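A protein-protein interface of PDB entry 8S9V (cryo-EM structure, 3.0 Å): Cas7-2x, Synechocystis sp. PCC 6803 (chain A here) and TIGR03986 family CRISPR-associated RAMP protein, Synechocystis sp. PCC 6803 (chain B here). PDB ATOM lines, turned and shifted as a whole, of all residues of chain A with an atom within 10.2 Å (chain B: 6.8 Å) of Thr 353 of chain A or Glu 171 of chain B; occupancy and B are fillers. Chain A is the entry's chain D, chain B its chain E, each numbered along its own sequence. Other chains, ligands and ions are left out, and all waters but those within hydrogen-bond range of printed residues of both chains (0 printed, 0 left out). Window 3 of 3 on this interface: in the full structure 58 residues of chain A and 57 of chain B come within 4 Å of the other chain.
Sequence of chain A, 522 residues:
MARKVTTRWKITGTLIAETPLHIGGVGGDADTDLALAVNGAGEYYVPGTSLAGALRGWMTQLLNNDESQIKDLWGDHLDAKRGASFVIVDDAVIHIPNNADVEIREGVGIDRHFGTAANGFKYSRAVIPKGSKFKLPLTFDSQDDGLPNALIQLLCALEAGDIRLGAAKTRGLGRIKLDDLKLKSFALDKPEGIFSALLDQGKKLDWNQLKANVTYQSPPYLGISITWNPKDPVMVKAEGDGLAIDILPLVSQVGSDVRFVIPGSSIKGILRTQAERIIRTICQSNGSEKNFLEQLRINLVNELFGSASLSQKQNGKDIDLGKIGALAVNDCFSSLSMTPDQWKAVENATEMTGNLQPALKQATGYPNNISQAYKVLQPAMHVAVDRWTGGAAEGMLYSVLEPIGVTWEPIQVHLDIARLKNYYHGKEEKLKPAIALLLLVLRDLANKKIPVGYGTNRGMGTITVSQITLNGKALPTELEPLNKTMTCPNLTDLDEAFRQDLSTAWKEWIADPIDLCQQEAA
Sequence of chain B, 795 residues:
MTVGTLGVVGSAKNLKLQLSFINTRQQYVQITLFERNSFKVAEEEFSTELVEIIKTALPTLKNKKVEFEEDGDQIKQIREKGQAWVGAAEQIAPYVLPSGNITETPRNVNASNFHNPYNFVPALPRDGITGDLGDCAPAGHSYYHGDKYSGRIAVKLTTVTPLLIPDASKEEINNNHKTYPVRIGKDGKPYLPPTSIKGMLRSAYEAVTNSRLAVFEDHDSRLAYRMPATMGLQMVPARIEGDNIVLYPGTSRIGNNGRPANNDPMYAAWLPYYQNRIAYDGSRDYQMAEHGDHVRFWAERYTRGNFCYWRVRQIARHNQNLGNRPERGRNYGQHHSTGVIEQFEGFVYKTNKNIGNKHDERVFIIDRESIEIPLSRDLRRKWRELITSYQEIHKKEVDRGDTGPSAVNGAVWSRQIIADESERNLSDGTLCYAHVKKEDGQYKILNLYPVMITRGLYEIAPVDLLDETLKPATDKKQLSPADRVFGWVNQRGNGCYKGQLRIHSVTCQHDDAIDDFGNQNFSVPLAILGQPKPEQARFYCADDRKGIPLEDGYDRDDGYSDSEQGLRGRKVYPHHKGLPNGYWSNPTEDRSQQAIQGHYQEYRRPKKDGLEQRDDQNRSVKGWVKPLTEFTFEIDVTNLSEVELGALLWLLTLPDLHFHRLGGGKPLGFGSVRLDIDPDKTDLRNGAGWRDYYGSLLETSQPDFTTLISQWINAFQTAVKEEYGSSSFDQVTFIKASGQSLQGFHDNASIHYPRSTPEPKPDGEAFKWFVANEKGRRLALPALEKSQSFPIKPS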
ATOM      1  N   LEU A 243      -4.198  -7.671  24.711  1.00  0.00           N
ATOM      2  CA  LEU A 243      -3.985  -9.119  24.709  1.00  0.00           C
ATOM      3  C   LEU A 243      -3.948  -9.682  23.291  1.00  0.00           C
ATOM      4  O   LEU A 243      -2.883 -10.056  22.795  1.00  0.00           O
ATOM      5  CB  LEU A 243      -5.070  -9.783  25.544  1.00  0.00           C
ATOM      6  CG  LEU A 243      -4.924  -9.445  27.023  1.00  0.00           C
ATOM      7  CD1 LEU A 243      -6.193  -9.796  27.755  1.00  0.00           C
ATOM      8  CD2 LEU A 243      -3.734 -10.158  27.633  1.00  0.00           C
ATOM      9  N   ALA A 244      -5.104  -9.788  22.640  1.00  0.00           N
ATOM     10  CA  ALA A 244      -5.098 -10.227  21.250  1.00  0.00           C
ATOM     11  C   ALA A 244      -4.486  -9.192  20.336  1.00  0.00           C
ATOM     12  O   ALA A 244      -3.904  -9.542  19.309  1.00  0.00           O
ATOM     13  CB  ALA A 244      -6.507 -10.543  20.777  1.00  0.00           C
ATOM     14  N   ILE A 245      -4.621  -7.921  20.683  1.00  0.00           N
ATOM     15  CA  ILE A 245      -4.111  -6.811  19.898  1.00  0.00           C
ATOM     16  C   ILE A 245      -3.194  -6.002  20.792  1.00  0.00           C
ATOM     17  O   ILE A 245      -3.585  -5.607  21.891  1.00  0.00           O
ATOM     18  CB  ILE A 245      -5.261  -5.937  19.384  1.00  0.00           C
ATOM     19  CG1 ILE A 245      -6.192  -6.729  18.487  1.00  0.00           C
ATOM     20  CG2 ILE A 245      -4.728  -4.826  18.606  1.00  0.00           C
ATOM     21  CD1 ILE A 245      -5.553  -7.190  17.259  1.00  0.00           C
ATOM     22  N   ALA A 349     -10.328  -9.524  24.402  1.00  0.00           N
ATOM     23  CA  ALA A 349     -10.140 -10.649  23.509  1.00  0.00           C
ATOM     24  C   ALA A 349      -8.713 -11.139  23.610  1.00  0.00           C
ATOM     25  O   ALA A 349      -7.813 -10.400  23.997  1.00  0.00           O
ATOM     26  CB  ALA A 349     -10.450 -10.261  22.073  1.00  0.00           C
ATOM     27  N   THR A 350      -8.524 -12.422  23.342  1.00  0.00           N
ATOM     28  CA  THR A 350      -7.225 -13.060  23.485  1.00  0.00           C
ATOM     29  C   THR A 350      -6.785 -13.851  22.268  1.00  0.00           C
ATOM     30  O   THR A 350      -5.598 -14.181  22.174  1.00  0.00           O
ATOM     31  CB  THR A 350      -7.183 -13.948  24.730  1.00  0.00           C
ATOM     32  OG1 THR A 350      -8.299 -14.837  24.732  1.00  0.00           O
ATOM     33  CG2 THR A 350      -7.207 -13.109  25.956  1.00  0.00           C
ATOM     34  N   GLU A 351      -7.682 -14.185  21.351  1.00  0.00           N
ATOM     35  CA  GLU A 351      -7.327 -14.896  20.133  1.00  0.00           C
ATOM     36  C   GLU A 351      -7.751 -14.041  18.953  1.00  0.00           C
ATOM     37  O   GLU A 351      -8.942 -13.797  18.764  1.00  0.00           O
ATOM     38  CB  GLU A 351      -8.035 -16.246  20.080  1.00  0.00           C
ATOM     39  CG  GLU A 351      -7.694 -17.153  21.247  1.00  0.00           C
ATOM     40  CD  GLU A 351      -6.231 -17.513  21.310  1.00  0.00           C
ATOM     41  OE1 GLU A 351      -5.597 -17.628  20.238  1.00  0.00           O
ATOM     42  OE2 GLU A 351      -5.715 -17.670  22.436  1.00  0.00           O
ATOM     43  N   MET A 352      -6.792 -13.639  18.128  1.00  0.00           N
ATOM     44  CA  MET A 352      -7.125 -12.733  17.040  1.00  0.00           C
ATOM     45  C   MET A 352      -8.105 -13.366  16.075  1.00  0.00           C
ATOM     46  O   MET A 352      -8.972 -12.681  15.529  1.00  0.00           O
ATOM     47  CB  MET A 352      -5.863 -12.288  16.310  1.00  0.00           C
ATOM     48  CG  MET A 352      -6.135 -11.336  15.190  1.00  0.00           C
ATOM     49  SD  MET A 352      -4.706 -10.904  14.218  1.00  0.00           S
ATOM     50  CE  MET A 352      -3.896  -9.821  15.369  1.00  0.00           C
ATOM     51  N   THR A 353      -7.978 -14.659  15.836  1.00  0.00           N
ATOM     52  CA  THR A 353      -8.929 -15.389  15.014  1.00  0.00           C
ATOM     53  C   THR A 353     -10.027 -16.046  15.824  1.00  0.00           C
ATOM     54  O   THR A 353     -10.957 -16.599  15.239  1.00  0.00           O
ATOM     55  CB  THR A 353      -8.216 -16.443  14.193  1.00  0.00           C
ATOM     56  OG1 THR A 353      -7.522 -17.328  15.073  1.00  0.00           O
ATOM     57  CG2 THR A 353      -7.226 -15.788  13.283  1.00  0.00           C
ATOM     58  N   GLY A 354      -9.931 -16.024  17.146  1.00  0.00           N
ATOM     59  CA  GLY A 354     -10.933 -16.625  17.992  1.00  0.00           C
ATOM     60  C   GLY A 354     -11.905 -15.630  18.569  1.00  0.00           C
ATOM     61  O   GLY A 354     -12.630 -14.969  17.831  1.00  0.00           O
ATOM     62  N   ASN A 355     -11.959 -15.548  19.894  1.00  0.00           N
ATOM     63  CA  ASN A 355     -12.933 -14.716  20.585  1.00  0.00           C
ATOM     64  C   ASN A 355     -12.837 -13.237  20.247  1.00  0.00           C
ATOM     65  O   ASN A 355     -13.733 -12.489  20.636  1.00  0.00           O
ATOM     66  CB  ASN A 355     -12.812 -14.902  22.082  1.00  0.00           C
ATOM     67  CG  ASN A 355     -11.460 -14.608  22.575  1.00  0.00           C
ATOM     68  OD1 ASN A 355     -10.728 -13.858  21.959  1.00  0.00           O
ATOM     69  ND2 ASN A 355     -11.093 -15.205  23.690  1.00  0.00           N
ATOM     70  N   LEU A 356     -11.776 -12.780  19.586  1.00  0.00           N
ATOM     71  CA  LEU A 356     -11.773 -11.409  19.084  1.00  0.00           C
ATOM     72  C   LEU A 356     -12.803 -11.188  17.996  1.00  0.00           C
ATOM     73  O   LEU A 356     -13.372 -10.104  17.897  1.00  0.00           O
ATOM     74  CB  LEU A 356     -10.404 -11.039  18.542  1.00  0.00           C
ATOM     75  CG  LEU A 356     -10.336  -9.591  18.086  1.00  0.00           C
ATOM     76  CD1 LEU A 356     -10.325  -8.680  19.287  1.00  0.00           C
ATOM     77  CD2 LEU A 356      -9.139  -9.357  17.218  1.00  0.00           C
ATOM     78  N   GLN A 357     -13.046 -12.179  17.156  1.00  0.00           N
ATOM     79  CA  GLN A 357     -13.962 -11.964  16.041  1.00  0.00           C
ATOM     80  C   GLN A 357     -15.384 -11.681  16.487  1.00  0.00           C
ATOM     81  O   GLN A 357     -15.994 -10.732  15.971  1.00  0.00           O
ATOM     82  CB  GLN A 357     -13.901 -13.147  15.082  1.00  0.00           C
ATOM     83  CG  GLN A 357     -12.553 -13.344  14.456  1.00  0.00           C
ATOM     84  CD  GLN A 357     -12.622 -14.264  13.272  1.00  0.00           C
ATOM     85  OE1 GLN A 357     -13.559 -15.038  13.136  1.00  0.00           O
ATOM     86  NE2 GLN A 357     -11.642 -14.172  12.392  1.00  0.00           N
ATOM     87  N   PRO A 358     -15.966 -12.426  17.416  1.00  0.00           N
ATOM     88  CA  PRO A 358     -17.250 -11.995  17.983  1.00  0.00           C
ATOM     89  C   PRO A 358     -17.241 -10.588  18.556  1.00  0.00           C
ATOM     90  O   PRO A 358     -18.188  -9.833  18.323  1.00  0.00           O
ATOM     91  CB  PRO A 358     -17.494 -13.042  19.072  1.00  0.00           C
ATOM     92  CG  PRO A 358     -16.795 -14.229  18.586  1.00  0.00           C
ATOM     93  CD  PRO A 358     -15.556 -13.735  17.934  1.00  0.00           C
ATOM     94  N   ALA A 359     -16.199 -10.208  19.291  1.00  0.00           N
ATOM     95  CA  ALA A 359     -16.158  -8.888  19.907  1.00  0.00           C
ATOM     96  C   ALA A 359     -16.170  -7.757  18.888  1.00  0.00           C
ATOM     97  O   ALA A 359     -16.881  -6.771  19.070  1.00  0.00           O
ATOM     98  CB  ALA A 359     -14.930  -8.774  20.798  1.00  0.00           C
ATOM     99  N   LEU A 360     -15.397  -7.868  17.814  1.00  0.00           N
ATOM    100  CA  LEU A 360     -15.406  -6.814  16.803  1.00  0.00           C
ATOM    101  C   LEU A 360     -16.684  -6.808  15.981  1.00  0.00           C
ATOM    102  O   LEU A 360     -17.145  -5.747  15.559  1.00  0.00           O
ATOM    103  CB  LEU A 360     -14.224  -6.963  15.857  1.00  0.00           C
ATOM    104  CG  LEU A 360     -12.820  -6.785  16.385  1.00  0.00           C
ATOM    105  CD1 LEU A 360     -11.888  -7.022  15.247  1.00  0.00           C
ATOM    106  CD2 LEU A 360     -12.617  -5.442  17.002  1.00  0.00           C
ATOM    107  N   LYS A 361     -17.249  -7.973  15.701  1.00  0.00           N
ATOM    108  CA  LYS A 361     -18.559  -8.008  15.070  1.00  0.00           C
ATOM    109  C   LYS A 361     -19.605  -7.305  15.921  1.00  0.00           C
ATOM    110  O   LYS A 361     -20.459  -6.587  15.397  1.00  0.00           O
ATOM    111  CB  LYS A 361     -18.964  -9.443  14.763  1.00  0.00           C
ATOM    112  CG  LYS A 361     -18.255 -10.005  13.567  1.00  0.00           C
ATOM    113  CD  LYS A 361     -18.830 -11.324  13.124  1.00  0.00           C
ATOM    114  CE  LYS A 361     -18.629 -12.413  14.131  1.00  0.00           C
ATOM    115  NZ  LYS A 361     -19.039 -13.714  13.547  1.00  0.00           N
ATOM    116  N   ILE A 370     -18.745 -10.438   9.427  1.00  0.00           N
ATOM    117  CA  ILE A 370     -17.387 -10.018   9.757  1.00  0.00           C
ATOM    118  C   ILE A 370     -16.747  -9.255   8.608  1.00  0.00           C
ATOM    119  O   ILE A 370     -15.928  -8.364   8.834  1.00  0.00           O
ATOM    120  CB  ILE A 370     -16.518 -11.210  10.159  1.00  0.00           C
ATOM    121  CG1 ILE A 370     -15.448 -10.747  11.127  1.00  0.00           C
ATOM    122  CG2 ILE A 370     -15.826 -11.763   8.956  1.00  0.00           C
ATOM    123  CD1 ILE A 370     -14.645 -11.848  11.696  1.00  0.00           C
ATOM    124  N   TYR A 374     -14.864  -5.900   9.622  1.00  0.00           N
ATOM    125  CA  TYR A 374     -13.480  -5.569   9.296  1.00  0.00           C
ATOM    126  C   TYR A 374     -13.323  -4.509   8.224  1.00  0.00           C
ATOM    127  O   TYR A 374     -12.205  -4.285   7.767  1.00  0.00           O
ATOM    128  CB  TYR A 374     -12.732  -6.823   8.871  1.00  0.00           C
ATOM    129  CG  TYR A 374     -12.494  -7.746  10.010  1.00  0.00           C
ATOM    130  CD1 TYR A 374     -12.873  -7.398  11.279  1.00  0.00           C
ATOM    131  CD2 TYR A 374     -11.881  -8.949   9.824  1.00  0.00           C
ATOM    132  CE1 TYR A 374     -12.682  -8.239  12.320  1.00  0.00           C
ATOM    133  CE2 TYR A 374     -11.669  -9.780  10.864  1.00  0.00           C
ATOM    134  CZ  TYR A 374     -12.080  -9.426  12.108  1.00  0.00           C
ATOM    135  OH  TYR A 374     -11.834 -10.261  13.156  1.00  0.00           O
ATOM    136  N   PRO A 379      -7.943  -5.782  12.217  1.00  0.00           N
ATOM    137  CA  PRO A 379      -6.660  -6.172  12.809  1.00  0.00           C
ATOM    138  C   PRO A 379      -5.583  -6.342  11.750  1.00  0.00           C
ATOM    139  O   PRO A 379      -5.799  -6.979  10.722  1.00  0.00           O
ATOM    140  CB  PRO A 379      -6.983  -7.496  13.498  1.00  0.00           C
ATOM    141  CG  PRO A 379      -8.426  -7.507  13.633  1.00  0.00           C
ATOM    142  CD  PRO A 379      -8.964  -6.801  12.455  1.00  0.00           C
ATOM    143  N   MET A 381      -1.389  -7.466  11.232  1.00  0.00           N
ATOM    144  CA  MET A 381      -0.173  -8.063  11.764  1.00  0.00           C
ATOM    145  C   MET A 381       1.036  -7.474  11.075  1.00  0.00           C
ATOM    146  O   MET A 381       0.986  -7.174   9.885  1.00  0.00           O
ATOM    147  CB  MET A 381      -0.147  -9.577  11.581  1.00  0.00           C
ATOM    148  CG  MET A 381      -0.739 -10.355  12.697  1.00  0.00           C
ATOM    149  SD  MET A 381       0.406 -10.299  14.059  1.00  0.00           S
ATOM    150  CE  MET A 381      -0.286 -11.537  15.119  1.00  0.00           C
ATOM    151  N   LEU A 397       7.060  -9.733  16.342  1.00  0.00           N
ATOM    152  CA  LEU A 397       5.738  -9.875  15.746  1.00  0.00           C
ATOM    153  C   LEU A 397       4.718  -9.092  16.562  1.00  0.00           C
ATOM    154  O   LEU A 397       4.644  -9.261  17.778  1.00  0.00           O
ATOM    155  CB  LEU A 397       5.361 -11.348  15.684  1.00  0.00           C
ATOM    156  CG  LEU A 397       4.030 -11.806  15.145  1.00  0.00           C
ATOM    157  CD1 LEU A 397       3.934 -11.448  13.719  1.00  0.00           C
ATOM    158  CD2 LEU A 397       3.950 -13.265  15.312  1.00  0.00           C
ATOM    159  N   SER A 399       0.762  -6.574  16.330  1.00  0.00           N
ATOM    160  CA  SER A 399      -0.502  -6.402  15.633  1.00  0.00           C
ATOM    161  C   SER A 399      -1.159  -5.109  16.070  1.00  0.00           C
ATOM    162  O   SER A 399      -0.946  -4.639  17.181  1.00  0.00           O
ATOM    163  CB  SER A 399      -1.436  -7.557  15.886  1.00  0.00           C
ATOM    164  OG  SER A 399      -1.791  -7.577  17.239  1.00  0.00           O
ATOM    165  N   ASP B 167      -4.487 -11.677   4.793  1.00  0.00           N
ATOM    166  CA  ASP B 167      -5.116 -11.093   5.975  1.00  0.00           C
ATOM    167  C   ASP B 167      -5.108 -12.136   7.081  1.00  0.00           C
ATOM    168  O   ASP B 167      -5.973 -13.005   7.133  1.00  0.00           O
ATOM    169  CB  ASP B 167      -6.539 -10.644   5.682  1.00  0.00           C
ATOM    170  CG  ASP B 167      -7.110  -9.772   6.780  1.00  0.00           C
ATOM    171  OD1 ASP B 167      -6.505  -9.691   7.862  1.00  0.00           O
ATOM    172  OD2 ASP B 167      -8.167  -9.156   6.565  1.00  0.00           O
ATOM    173  N   ALA B 168      -4.124 -12.043   7.969  1.00  0.00           N
ATOM    174  CA  ALA B 168      -4.014 -12.927   9.117  1.00  0.00           C
ATOM    175  C   ALA B 168      -5.128 -12.754  10.140  1.00  0.00           C
ATOM    176  O   ALA B 168      -5.201 -13.549  11.079  1.00  0.00           O
ATOM    177  CB  ALA B 168      -2.668 -12.719   9.790  1.00  0.00           C
ATOM    178  N   SER B 169      -5.955 -11.723  10.024  1.00  0.00           N
ATOM    179  CA  SER B 169      -7.133 -11.589  10.875  1.00  0.00           C
ATOM    180  C   SER B 169      -8.287 -12.482  10.454  1.00  0.00           C
ATOM    181  O   SER B 169      -9.138 -12.818  11.277  1.00  0.00           O
ATOM    182  CB  SER B 169      -7.598 -10.146  10.863  1.00  0.00           C
ATOM    183  OG  SER B 169      -8.222  -9.856   9.628  1.00  0.00           O
ATOM    184  N   LYS B 170      -8.351 -12.834   9.178  1.00  0.00           N
ATOM    185  CA  LYS B 170      -9.418 -13.622   8.588  1.00  0.00           C
ATOM    186  C   LYS B 170      -8.979 -15.034   8.230  1.00  0.00           C
ATOM    187  O   LYS B 170      -9.751 -15.769   7.613  1.00  0.00           O
ATOM    188  CB  LYS B 170      -9.936 -12.885   7.359  1.00  0.00           C
ATOM    189  CG  LYS B 170     -10.651 -11.590   7.709  1.00  0.00           C
ATOM    190  CD  LYS B 170     -11.109 -10.835   6.475  1.00  0.00           C
ATOM    191  CE  LYS B 170     -12.143 -11.552   5.688  1.00  0.00           C
ATOM    192  NZ  LYS B 170     -12.456 -10.738   4.495  1.00  0.00           N
ATOM    193  N   GLU B 171      -7.762 -15.423   8.597  1.00  0.00           N
ATOM    194  CA  GLU B 171      -7.249 -16.749   8.282  1.00  0.00           C
ATOM    195  C   GLU B 171      -8.140 -17.826   8.872  1.00  0.00           C
ATOM    196  O   GLU B 171      -8.808 -17.627   9.886  1.00  0.00           O
ATOM    197  CB  GLU B 171      -5.857 -16.957   8.841  1.00  0.00           C
ATOM    198  CG  GLU B 171      -5.881 -17.160  10.318  1.00  0.00           C
ATOM    199  CD  GLU B 171      -4.527 -17.469  10.883  1.00  0.00           C
ATOM    200  OE1 GLU B 171      -3.557 -16.770  10.541  1.00  0.00           O
ATOM    201  OE2 GLU B 171      -4.428 -18.440  11.653  1.00  0.00           O
ATOM    202  N   GLU B 172      -8.149 -18.980   8.220  1.00  0.00           N
ATOM    203  CA  GLU B 172      -8.960 -20.113   8.624  1.00  0.00           C
ATOM    204  C   GLU B 172      -8.062 -21.321   8.832  1.00  0.00           C
ATOM    205  O   GLU B 172      -7.155 -21.569   8.037  1.00  0.00           O
ATOM    206  CB  GLU B 172      -9.967 -20.421   7.539  1.00  0.00           C
ATOM    207  CG  GLU B 172     -10.952 -19.327   7.315  1.00  0.00           C
ATOM    208  CD  GLU B 172     -12.016 -19.731   6.346  1.00  0.00           C
ATOM    209  OE1 GLU B 172     -11.649 -20.089   5.208  1.00  0.00           O
ATOM    210  OE2 GLU B 172     -13.210 -19.684   6.706  1.00  0.00           O
ATOM    211  N   ILE B 173      -8.335 -22.092   9.878  1.00  0.00           N
ATOM    212  CA  ILE B 173      -7.475 -23.191  10.291  1.00  0.00           C
ATOM    213  C   ILE B 173      -8.264 -24.484  10.190  1.00  0.00           C
ATOM    214  O   ILE B 173      -9.309 -24.626  10.833  1.00  0.00           O
ATOM    215  CB  ILE B 173      -6.953 -23.000  11.720  1.00  0.00           C
ATOM    216  CG1 ILE B 173      -6.236 -21.669  11.854  1.00  0.00           C
ATOM    217  CG2 ILE B 173      -5.996 -24.084  12.071  1.00  0.00           C
ATOM    218  CD1 ILE B 173      -7.103 -20.549  12.346  1.00  0.00           C
ATOM    219  N   LYS B 178      -3.419 -23.352   7.583  1.00  0.00           N
ATOM    220  CA  LYS B 178      -3.957 -21.992   7.576  1.00  0.00           C
ATOM    221  C   LYS B 178      -4.215 -21.501   6.162  1.00  0.00           C
ATOM    222  O   LYS B 178      -3.310 -21.504   5.328  1.00  0.00           O
ATOM    223  CB  LYS B 178      -3.017 -21.015   8.262  1.00  0.00           C
ATOM    224  CG  LYS B 178      -2.819 -21.207   9.726  1.00  0.00           C
ATOM    225  CD  LYS B 178      -1.825 -20.185  10.173  1.00  0.00           C
ATOM    226  CE  LYS B 178      -1.467 -20.292  11.621  1.00  0.00           C
ATOM    227  NZ  LYS B 178      -2.613 -19.875  12.449  1.00  0.00           N
ATOM    228  N   THR B 179      -5.435 -21.044   5.909  1.00  0.00           N
ATOM    229  CA  THR B 179      -5.845 -20.470   4.633  1.00  0.00           C
ATOM    230  C   THR B 179      -6.022 -18.971   4.784  1.00  0.00           C
ATOM    231  O   THR B 179      -6.637 -18.518   5.751  1.00  0.00           O
ATOM    232  CB  THR B 179      -7.150 -21.084   4.149  1.00  0.00           C
ATOM    233  OG1 THR B 179      -7.019 -22.506   4.097  1.00  0.00           O
ATOM    234  CG2 THR B 179      -7.478 -20.580   2.794  1.00  0.00           C
ATOM    235  N   TYR B 180      -5.447 -18.200   3.870  1.00  0.00           N
ATOM    236  CA  TYR B 180      -5.497 -16.760   3.994  1.00  0.00           C
ATOM    237  C   TYR B 180      -6.288 -16.172   2.834  1.00  0.00           C
ATOM    238  O   TYR B 180      -6.012 -16.505   1.678  1.00  0.00           O
ATOM    239  CB  TYR B 180      -4.100 -16.177   4.001  1.00  0.00           C
ATOM    240  CG  TYR B 180      -3.305 -16.496   5.232  1.00  0.00           C
ATOM    241  CD1 TYR B 180      -3.353 -15.704   6.337  1.00  0.00           C
ATOM    242  CD2 TYR B 180      -2.466 -17.578   5.257  1.00  0.00           C
ATOM    243  CE1 TYR B 180      -2.593 -15.975   7.411  1.00  0.00           C
ATOM    244  CE2 TYR B 180      -1.735 -17.871   6.348  1.00  0.00           C
ATOM    245  CZ  TYR B 180      -1.793 -17.061   7.411  1.00  0.00           C
ATOM    246  OH  TYR B 180      -1.074 -17.386   8.515  1.00  0.00           O
ATOM    247  N   PRO B 181      -7.238 -15.285   3.086  1.00  0.00           N
ATOM    248  CA  PRO B 181      -7.763 -14.419   2.033  1.00  0.00           C
ATOM    249  C   PRO B 181      -6.881 -13.204   1.796  1.00  0.00           C
ATOM    250  O   PRO B 181      -5.955 -12.926   2.545  1.00  0.00           O
ATOM    251  CB  PRO B 181      -9.115 -14.019   2.594  1.00  0.00           C
ATOM    252  CG  PRO B 181      -8.878 -13.950   4.044  1.00  0.00           C
ATOM    253  CD  PRO B 181      -7.862 -14.990   4.379  1.00  0.00           C
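O of Ser 169 of chain B sits at hydrogen-bond distance from NE2 of Gln 357 of chain A, at 3.1 Å.
Along chain B the printed residues that touch a printed residue of chain A span positions 168 to 171. Of the 22 printed residues of chain A, 4 touch a printed residue of chain B. Hydrophobic or aromatic side chains of chain A that line the printed part of chain B: Tyr 374 and Pro 379. Among the printed residues, no Asp or Glu carboxylate lies within 4 Å of a Lys or Arg side-chain nitrogen of the other chain.
Thr 353 of chain A touches just these residues of chain B: Ala 168 (3.7 Å) and Glu 171 (3.5 Å). Of chain A, only Thr 353 comes within 4 Å of Glu 171 of chain B. Ala 168 of chain B touches just one residue of chain A: Thr 353. No residue of chain A comes within 4 Å of Glu 172 of chain B. Printed residues of chain B within 4 Å of Tyr 374 of chain A: Ser 169 and Lys 170. Of the printed residues of chain A, Lys 170 of chain B touches Tyr 374 (3.6 Å). Of the printed residues of chain B, Pro 379 of chain A touches Ser 169. Of the printed residues of chain B, Gln 357 of chain A touches Ser 169 (3.1 Å). Met 352 of chain A touches none of the printed residues of chain B. The nearest residue of chain A that does not touch Glu 171 of chain B is Gln 357 of chain A (5.1 Å). The nearest printed residue of chain B that does not touch Pro 379 of chain A is Asp 167 of chain B (4.004 Å).
Among the printed residues, pairs that only touch across the chains: Thr 353 of chain A with Glu 171 of chain B, Tyr 374 of chain A with Lys 170 of chain B, Pro 379 of chain A with Ser 169 of chain B, Tyr 374 of chain A with Ser 169 of chain B and Thr 353 of chain A with Ala 168 of chain B.
OD1 of Asp 167 of chain B lies within hydrogen-bond range of OG of Ser 169 of chain B. The side-chain carboxylate (OE2) of Glu 171 of chain B is in salt-bridge range of the side-chain amino group (NZ) of Lys 178 of chain B, at 2.4 Å. The side-chain carboxylate (OE1) of Glu 171 of chain B is in hydrogen-bond range of the side-chain hydroxyl (OH) of Tyr 180 of chain B (3.3 Å).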
